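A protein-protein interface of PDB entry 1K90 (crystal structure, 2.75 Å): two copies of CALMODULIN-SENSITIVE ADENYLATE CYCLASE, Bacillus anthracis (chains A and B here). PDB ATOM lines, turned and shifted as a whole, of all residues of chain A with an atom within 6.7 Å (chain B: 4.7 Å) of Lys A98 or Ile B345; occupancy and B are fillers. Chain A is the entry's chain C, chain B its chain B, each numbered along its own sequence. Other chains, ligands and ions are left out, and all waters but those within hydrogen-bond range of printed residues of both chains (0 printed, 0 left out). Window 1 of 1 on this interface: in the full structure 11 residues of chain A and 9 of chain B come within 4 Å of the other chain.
Lys A98 touches Ile B345.
CB of Tyr B352 touches CD of Lys A98 (3.2 Å).
CG of Lys A99 touches CD1 of Ile B345, at 3.8 Å.
Thr A102 touches Ile B345 (OG1 to CD1, 3.6 Å).
CG2 of Thr A102 touches CE1 of Tyr B352 (3.7 Å).
The backbone carbonyl oxygen (O) of Pro B347 sits at hydrogen-bond distance from the side-chain amino group (NZ) of Lys B350 (2.9 Å).
The side-chain carboxylate of Glu A96 lies within salt-bridge range of the side-chain amino group of Lys A99 (3.7 Å).
OG1 of Thr A102 lies within hydrogen-bond range of O of Lys A98, at 2.8 Å.
O of Lys A99 sits at hydrogen-bond distance from OG1 of Thr A102 (3.2 Å).
Glu A96 touches none of the printed residues of chain B.
Lys A98 touches just these residues of chain B: Ile B345, Lys B350 and Tyr B352.
Of the printed residues of chain B, Lys A99 touches Ile B345 (3.8 Å).
Of the printed residues of chain B, Thr A102 touches Ile B345 (3.6 Å) and Tyr B352 (3.7 Å).
Ala B351 touches none of the printed residues of chain A.
O of Lys B350 lies within hydrogen-bond range of NZ of Lys A98, at 3.0 Å.
No position is printed for both chains.
Of the 14 printed residues of chain A, 3 touch a printed residue of chain B.
Hydrophobic or aromatic side chains of chain B that line the printed part of chain A: Ile B345 and Tyr B352.
Along chain B the printed residues that touch a printed residue of chain A span positions 345 to 352.
Among the printed residues, 6 pairs touch across the chains.
Among the printed residues, no Asp or Glu carboxylate lies within 4 Å of a Lys or Arg side-chain nitrogen of the other chain.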
ATOM      1  N   PHE A  76       0.210 -16.859  13.095  1.00  0.00           N
ATOM      2  CA  PHE A  76       1.082 -17.541  14.029  1.00  0.00           C
ATOM      3  C   PHE A  76       2.519 -17.187  13.679  1.00  0.00           C
ATOM      4  O   PHE A  76       3.262 -16.684  14.518  1.00  0.00           O
ATOM      5  CB  PHE A  76       0.872 -19.047  13.945  1.00  0.00           C
ATOM      6  CG  PHE A  76       1.671 -19.817  14.947  1.00  0.00           C
ATOM      7  CD1 PHE A  76       1.578 -19.518  16.299  1.00  0.00           C
ATOM      8  CD2 PHE A  76       2.520 -20.835  14.543  1.00  0.00           C
ATOM      9  CE1 PHE A  76       2.320 -20.219  17.238  1.00  0.00           C
ATOM     10  CE2 PHE A  76       3.265 -21.543  15.469  1.00  0.00           C
ATOM     11  CZ  PHE A  76       3.166 -21.233  16.824  1.00  0.00           C
ATOM     12  N   GLU A  91      10.548 -12.266  16.005  1.00  0.00           N
ATOM     13  CA  GLU A  91      10.922 -13.221  17.036  1.00  0.00           C
ATOM     14  C   GLU A  91      10.008 -13.021  18.245  1.00  0.00           C
ATOM     15  O   GLU A  91       9.301 -13.945  18.652  1.00  0.00           O
ATOM     16  CB  GLU A  91      12.377 -13.019  17.449  1.00  0.00           C
ATOM     17  CG  GLU A  91      13.136 -14.313  17.656  1.00  0.00           C
ATOM     18  CD  GLU A  91      13.898 -14.735  16.418  1.00  0.00           C
ATOM     19  OE1 GLU A  91      13.273 -14.833  15.343  1.00  0.00           O
ATOM     20  OE2 GLU A  91      15.122 -14.965  16.522  1.00  0.00           O
ATOM     21  N   GLY A  93       7.448 -11.818  18.310  1.00  0.00           N
ATOM     22  CA  GLY A  93       6.117 -12.144  17.857  1.00  0.00           C
ATOM     23  C   GLY A  93       5.812 -13.612  18.043  1.00  0.00           C
ATOM     24  O   GLY A  93       4.928 -13.979  18.812  1.00  0.00           O
ATOM     25  N   ASN A  94       6.564 -14.457  17.348  1.00  0.00           N
ATOM     26  CA  ASN A  94       6.341 -15.887  17.424  1.00  0.00           C
ATOM     27  C   ASN A  94       6.364 -16.407  18.850  1.00  0.00           C
ATOM     28  O   ASN A  94       5.494 -17.185  19.244  1.00  0.00           O
ATOM     29  CB  ASN A  94       7.374 -16.624  16.580  1.00  0.00           C
ATOM     30  CG  ASN A  94       7.387 -16.150  15.144  1.00  0.00           C
ATOM     31  OD1 ASN A  94       6.339 -15.904  14.554  1.00  0.00           O
ATOM     32  ND2 ASN A  94       8.575 -16.032  14.572  1.00  0.00           N
ATOM     33  N   LEU A  95       7.349 -15.974  19.628  1.00  0.00           N
ATOM     34  CA  LEU A  95       7.453 -16.426  21.006  1.00  0.00           C
ATOM     35  C   LEU A  95       6.207 -16.023  21.787  1.00  0.00           C
ATOM     36  O   LEU A  95       5.744 -16.750  22.668  1.00  0.00           O
ATOM     37  CB  LEU A  95       8.716 -15.852  21.661  1.00  0.00           C
ATOM     38  CG  LEU A  95       9.092 -16.247  23.102  1.00  0.00           C
ATOM     39  CD1 LEU A  95       8.550 -15.233  24.084  1.00  0.00           C
ATOM     40  CD2 LEU A  95       8.576 -17.639  23.423  1.00  0.00           C
ATOM     41  N   GLU A  96       5.649 -14.865  21.460  1.00  0.00           N
ATOM     42  CA  GLU A  96       4.455 -14.423  22.156  1.00  0.00           C
ATOM     43  C   GLU A  96       3.290 -15.314  21.730  1.00  0.00           C
ATOM     44  O   GLU A  96       2.508 -15.764  22.565  1.00  0.00           O
ATOM     45  CB  GLU A  96       4.162 -12.954  21.843  1.00  0.00           C
ATOM     46  CG  GLU A  96       3.333 -12.290  22.917  1.00  0.00           C
ATOM     47  CD  GLU A  96       4.041 -12.251  24.256  1.00  0.00           C
ATOM     48  OE1 GLU A  96       3.379 -11.985  25.279  1.00  0.00           O
ATOM     49  OE2 GLU A  96       5.268 -12.478  24.285  1.00  0.00           O
ATOM     50  N   ASN A  97       3.187 -15.581  20.431  1.00  0.00           N
ATOM     51  CA  ASN A  97       2.129 -16.447  19.920  1.00  0.00           C
ATOM     52  C   ASN A  97       2.242 -17.849  20.511  1.00  0.00           C
ATOM     53  O   ASN A  97       1.239 -18.516  20.725  1.00  0.00           O
ATOM     54  CB  ASN A  97       2.198 -16.566  18.398  1.00  0.00           C
ATOM     55  CG  ASN A  97       1.667 -15.348  17.695  1.00  0.00           C
ATOM     56  OD1 ASN A  97       0.648 -14.787  18.093  1.00  0.00           O
ATOM     57  ND2 ASN A  97       2.343 -14.937  16.627  1.00  0.00           N
ATOM     58  N   LYS A  98       3.470 -18.295  20.760  1.00  0.00           N
ATOM     59  CA  LYS A  98       3.692 -19.620  21.315  1.00  0.00           C
ATOM     60  C   LYS A  98       3.255 -19.719  22.762  1.00  0.00           C
ATOM     61  O   LYS A  98       2.718 -20.741  23.179  1.00  0.00           O
ATOM     62  CB  LYS A  98       5.160 -20.022  21.162  1.00  0.00           C
ATOM     63  CG  LYS A  98       5.456 -20.584  19.775  1.00  0.00           C
ATOM     64  CD  LYS A  98       6.934 -20.862  19.520  1.00  0.00           C
ATOM     65  CE  LYS A  98       7.694 -19.595  19.162  1.00  0.00           C
ATOM     66  NZ  LYS A  98       9.004 -19.905  18.522  1.00  0.00           N
ATOM     67  N   LYS A  99       3.473 -18.663  23.535  1.00  0.00           N
ATOM     68  CA  LYS A  99       3.051 -18.681  24.928  1.00  0.00           C
ATOM     69  C   LYS A  99       1.526 -18.646  24.970  1.00  0.00           C
ATOM     70  O   LYS A  99       0.915 -19.274  25.825  1.00  0.00           O
ATOM     71  CB  LYS A  99       3.642 -17.489  25.689  1.00  0.00           C
ATOM     72  CG  LYS A  99       5.160 -17.564  25.836  1.00  0.00           C
ATOM     73  CD  LYS A  99       5.813 -16.196  26.006  1.00  0.00           C
ATOM     74  CE  LYS A  99       5.409 -15.507  27.298  1.00  0.00           C
ATOM     75  NZ  LYS A  99       6.095 -14.190  27.452  1.00  0.00           N
ATOM     76  N   SER A 100       0.910 -17.928  24.032  1.00  0.00           N
ATOM     77  CA  SER A 100      -0.552 -17.846  23.983  1.00  0.00           C
ATOM     78  C   SER A 100      -1.194 -19.209  23.764  1.00  0.00           C
ATOM     79  O   SER A 100      -2.246 -19.502  24.325  1.00  0.00           O
ATOM     80  CB  SER A 100      -1.013 -16.908  22.867  1.00  0.00           C
ATOM     81  OG  SER A 100      -0.951 -15.554  23.265  1.00  0.00           O
ATOM     82  N   ILE A 101      -0.556 -20.031  22.934  1.00  0.00           N
ATOM     83  CA  ILE A 101      -1.050 -21.369  22.619  1.00  0.00           C
ATOM     84  C   ILE A 101      -0.843 -22.320  23.790  1.00  0.00           C
ATOM     85  O   ILE A 101      -1.647 -23.221  24.020  1.00  0.00           O
ATOM     86  CB  ILE A 101      -0.309 -21.973  21.398  1.00  0.00           C
ATOM     87  CG1 ILE A 101      -0.439 -21.051  20.187  1.00  0.00           C
ATOM     88  CG2 ILE A 101      -0.871 -23.344  21.072  1.00  0.00           C
ATOM     89  CD1 ILE A 101      -1.857 -20.668  19.855  1.00  0.00           C
ATOM     90  N   THR A 102       0.242 -22.111  24.525  1.00  0.00           N
ATOM     91  CA  THR A 102       0.588 -22.959  25.658  1.00  0.00           C
ATOM     92  C   THR A 102       0.077 -22.468  27.014  1.00  0.00           C
ATOM     93  O   THR A 102      -0.700 -23.157  27.677  1.00  0.00           O
ATOM     94  CB  THR A 102       2.116 -23.143  25.735  1.00  0.00           C
ATOM     95  OG1 THR A 102       2.755 -21.863  25.743  1.00  0.00           O
ATOM     96  CG2 THR A 102       2.617 -23.923  24.531  1.00  0.00           C
ATOM     97  N   GLU A 103       0.511 -21.281  27.425  1.00  0.00           N
ATOM     98  CA  GLU A 103       0.106 -20.711  28.706  1.00  0.00           C
ATOM     99  C   GLU A 103      -1.410 -20.597  28.881  1.00  0.00           C
ATOM    100  O   GLU A 103      -1.936 -20.860  29.963  1.00  0.00           O
ATOM    101  CB  GLU A 103       0.761 -19.346  28.897  1.00  0.00           C
ATOM    102  CG  GLU A 103       2.287 -19.394  28.889  1.00  0.00           C
ATOM    103  CD  GLU A 103       2.923 -18.022  29.038  1.00  0.00           C
ATOM    104  OE1 GLU A 103       4.171 -17.942  29.020  1.00  0.00           O
ATOM    105  OE2 GLU A 103       2.181 -17.025  29.172  1.00  0.00           O
ATOM    106  N   MET A 187      -4.123 -17.012  14.723  1.00  0.00           N
ATOM    107  CA  MET A 187      -4.443 -17.080  16.143  1.00  0.00           C
ATOM    108  C   MET A 187      -5.945 -17.065  16.374  1.00  0.00           C
ATOM    109  O   MET A 187      -6.629 -16.111  16.008  1.00  0.00           O
ATOM    110  CB  MET A 187      -3.800 -15.897  16.875  1.00  0.00           C
ATOM    111  CG  MET A 187      -2.286 -15.900  16.849  1.00  0.00           C
ATOM    112  SD  MET A 187      -1.587 -17.098  17.968  1.00  0.00           S
ATOM    113  CE  MET A 187      -1.398 -18.413  16.872  1.00  0.00           C
ATOM    114  N   SER B 341      10.757 -32.085  24.568  1.00  0.00           N
ATOM    115  CA  SER B 341      10.450 -30.667  24.429  1.00  0.00           C
ATOM    116  C   SER B 341       9.352 -30.423  23.416  1.00  0.00           C
ATOM    117  O   SER B 341       8.683 -29.397  23.467  1.00  0.00           O
ATOM    118  CB  SER B 341      11.695 -29.864  24.064  1.00  0.00           C
ATOM    119  OG  SER B 341      12.314 -29.370  25.240  1.00  0.00           O
ATOM    120  N   LYS B 344       5.821 -28.267  23.193  1.00  0.00           N
ATOM    121  CA  LYS B 344       6.080 -27.407  24.338  1.00  0.00           C
ATOM    122  C   LYS B 344       7.077 -26.366  23.840  1.00  0.00           C
ATOM    123  O   LYS B 344       7.636 -26.516  22.748  1.00  0.00           O
ATOM    124  CB  LYS B 344       6.706 -28.228  25.478  1.00  0.00           C
ATOM    125  CG  LYS B 344       5.944 -29.515  25.799  1.00  0.00           C
ATOM    126  CD  LYS B 344       6.692 -30.431  26.764  1.00  0.00           C
ATOM    127  CE  LYS B 344       6.747 -29.863  28.175  1.00  0.00           C
ATOM    128  NZ  LYS B 344       7.454 -30.783  29.116  1.00  0.00           N
ATOM    129  N   ILE B 345       7.297 -25.311  24.613  1.00  0.00           N
ATOM    130  CA  ILE B 345       8.272 -24.301  24.205  1.00  0.00           C
ATOM    131  C   ILE B 345       9.660 -24.688  24.722  1.00  0.00           C
ATOM    132  O   ILE B 345       9.940 -24.562  25.914  1.00  0.00           O
ATOM    133  CB  ILE B 345       7.933 -22.910  24.763  1.00  0.00           C
ATOM    134  CG1 ILE B 345       6.528 -22.496  24.329  1.00  0.00           C
ATOM    135  CG2 ILE B 345       8.956 -21.894  24.260  1.00  0.00           C
ATOM    136  CD1 ILE B 345       6.130 -21.112  24.802  1.00  0.00           C
ATOM    137  N   ALA B 346      10.523 -25.163  23.828  1.00  0.00           N
ATOM    138  CA  ALA B 346      11.877 -25.561  24.204  1.00  0.00           C
ATOM    139  C   ALA B 346      12.552 -24.448  24.999  1.00  0.00           C
ATOM    140  O   ALA B 346      12.652 -23.310  24.545  1.00  0.00           O
ATOM    141  CB  ALA B 346      12.681 -25.892  22.961  1.00  0.00           C
ATOM    142  N   PRO B 347      13.028 -24.772  26.206  1.00  0.00           N
ATOM    143  CA  PRO B 347      13.696 -23.845  27.122  1.00  0.00           C
ATOM    144  C   PRO B 347      14.867 -23.056  26.546  1.00  0.00           C
ATOM    145  O   PRO B 347      15.108 -21.917  26.939  1.00  0.00           O
ATOM    146  CB  PRO B 347      14.133 -24.754  28.266  1.00  0.00           C
ATOM    147  CG  PRO B 347      13.103 -25.819  28.259  1.00  0.00           C
ATOM    148  CD  PRO B 347      12.982 -26.120  26.790  1.00  0.00           C
ATOM    149  N   LYS B 350      13.643 -21.680  22.472  1.00  0.00           N
ATOM    150  CA  LYS B 350      12.233 -21.302  22.472  1.00  0.00           C
ATOM    151  C   LYS B 350      11.517 -21.827  21.230  1.00  0.00           C
ATOM    152  O   LYS B 350      10.704 -21.132  20.626  1.00  0.00           O
ATOM    153  CB  LYS B 350      12.120 -19.783  22.522  1.00  0.00           C
ATOM    154  CG  LYS B 350      12.743 -19.147  23.761  1.00  0.00           C
ATOM    155  CD  LYS B 350      11.893 -19.383  24.994  1.00  0.00           C
ATOM    156  CE  LYS B 350      12.525 -18.755  26.224  1.00  0.00           C
ATOM    157  NZ  LYS B 350      13.870 -19.338  26.503  1.00  0.00           N
ATOM    158  N   ALA B 351      11.825 -23.059  20.851  1.00  0.00           N
ATOM    159  CA  ALA B 351      11.217 -23.667  19.683  1.00  0.00           C
ATOM    160  C   ALA B 351       9.995 -24.475  20.052  1.00  0.00           C
ATOM    161  O   ALA B 351       9.993 -25.231  21.029  1.00  0.00           O
ATOM    162  CB  ALA B 351      12.225 -24.563  18.967  1.00  0.00           C
ATOM    163  N   TYR B 352       8.952 -24.315  19.253  1.00  0.00           N
ATOM    164  CA  TYR B 352       7.720 -25.041  19.477  1.00  0.00           C
ATOM    165  C   TYR B 352       7.576 -26.051  18.347  1.00  0.00           C
ATOM    166  O   TYR B 352       6.984 -25.760  17.306  1.00  0.00           O
ATOM    167  CB  TYR B 352       6.538 -24.076  19.480  1.00  0.00           C
ATOM    168  CG  TYR B 352       5.232 -24.711  19.873  1.00  0.00           C
ATOM    169  CD1 TYR B 352       4.991 -25.093  21.186  1.00  0.00           C
ATOM    170  CD2 TYR B 352       4.237 -24.943  18.924  1.00  0.00           C
ATOM    171  CE1 TYR B 352       3.789 -25.688  21.551  1.00  0.00           C
ATOM    172  CE2 TYR B 352       3.036 -25.539  19.274  1.00  0.00           C
ATOM    173  CZ  TYR B 352       2.815 -25.909  20.587  1.00  0.00           C
ATOM    174  OH  TYR B 352       1.617 -26.491  20.946  1.00  0.00           O
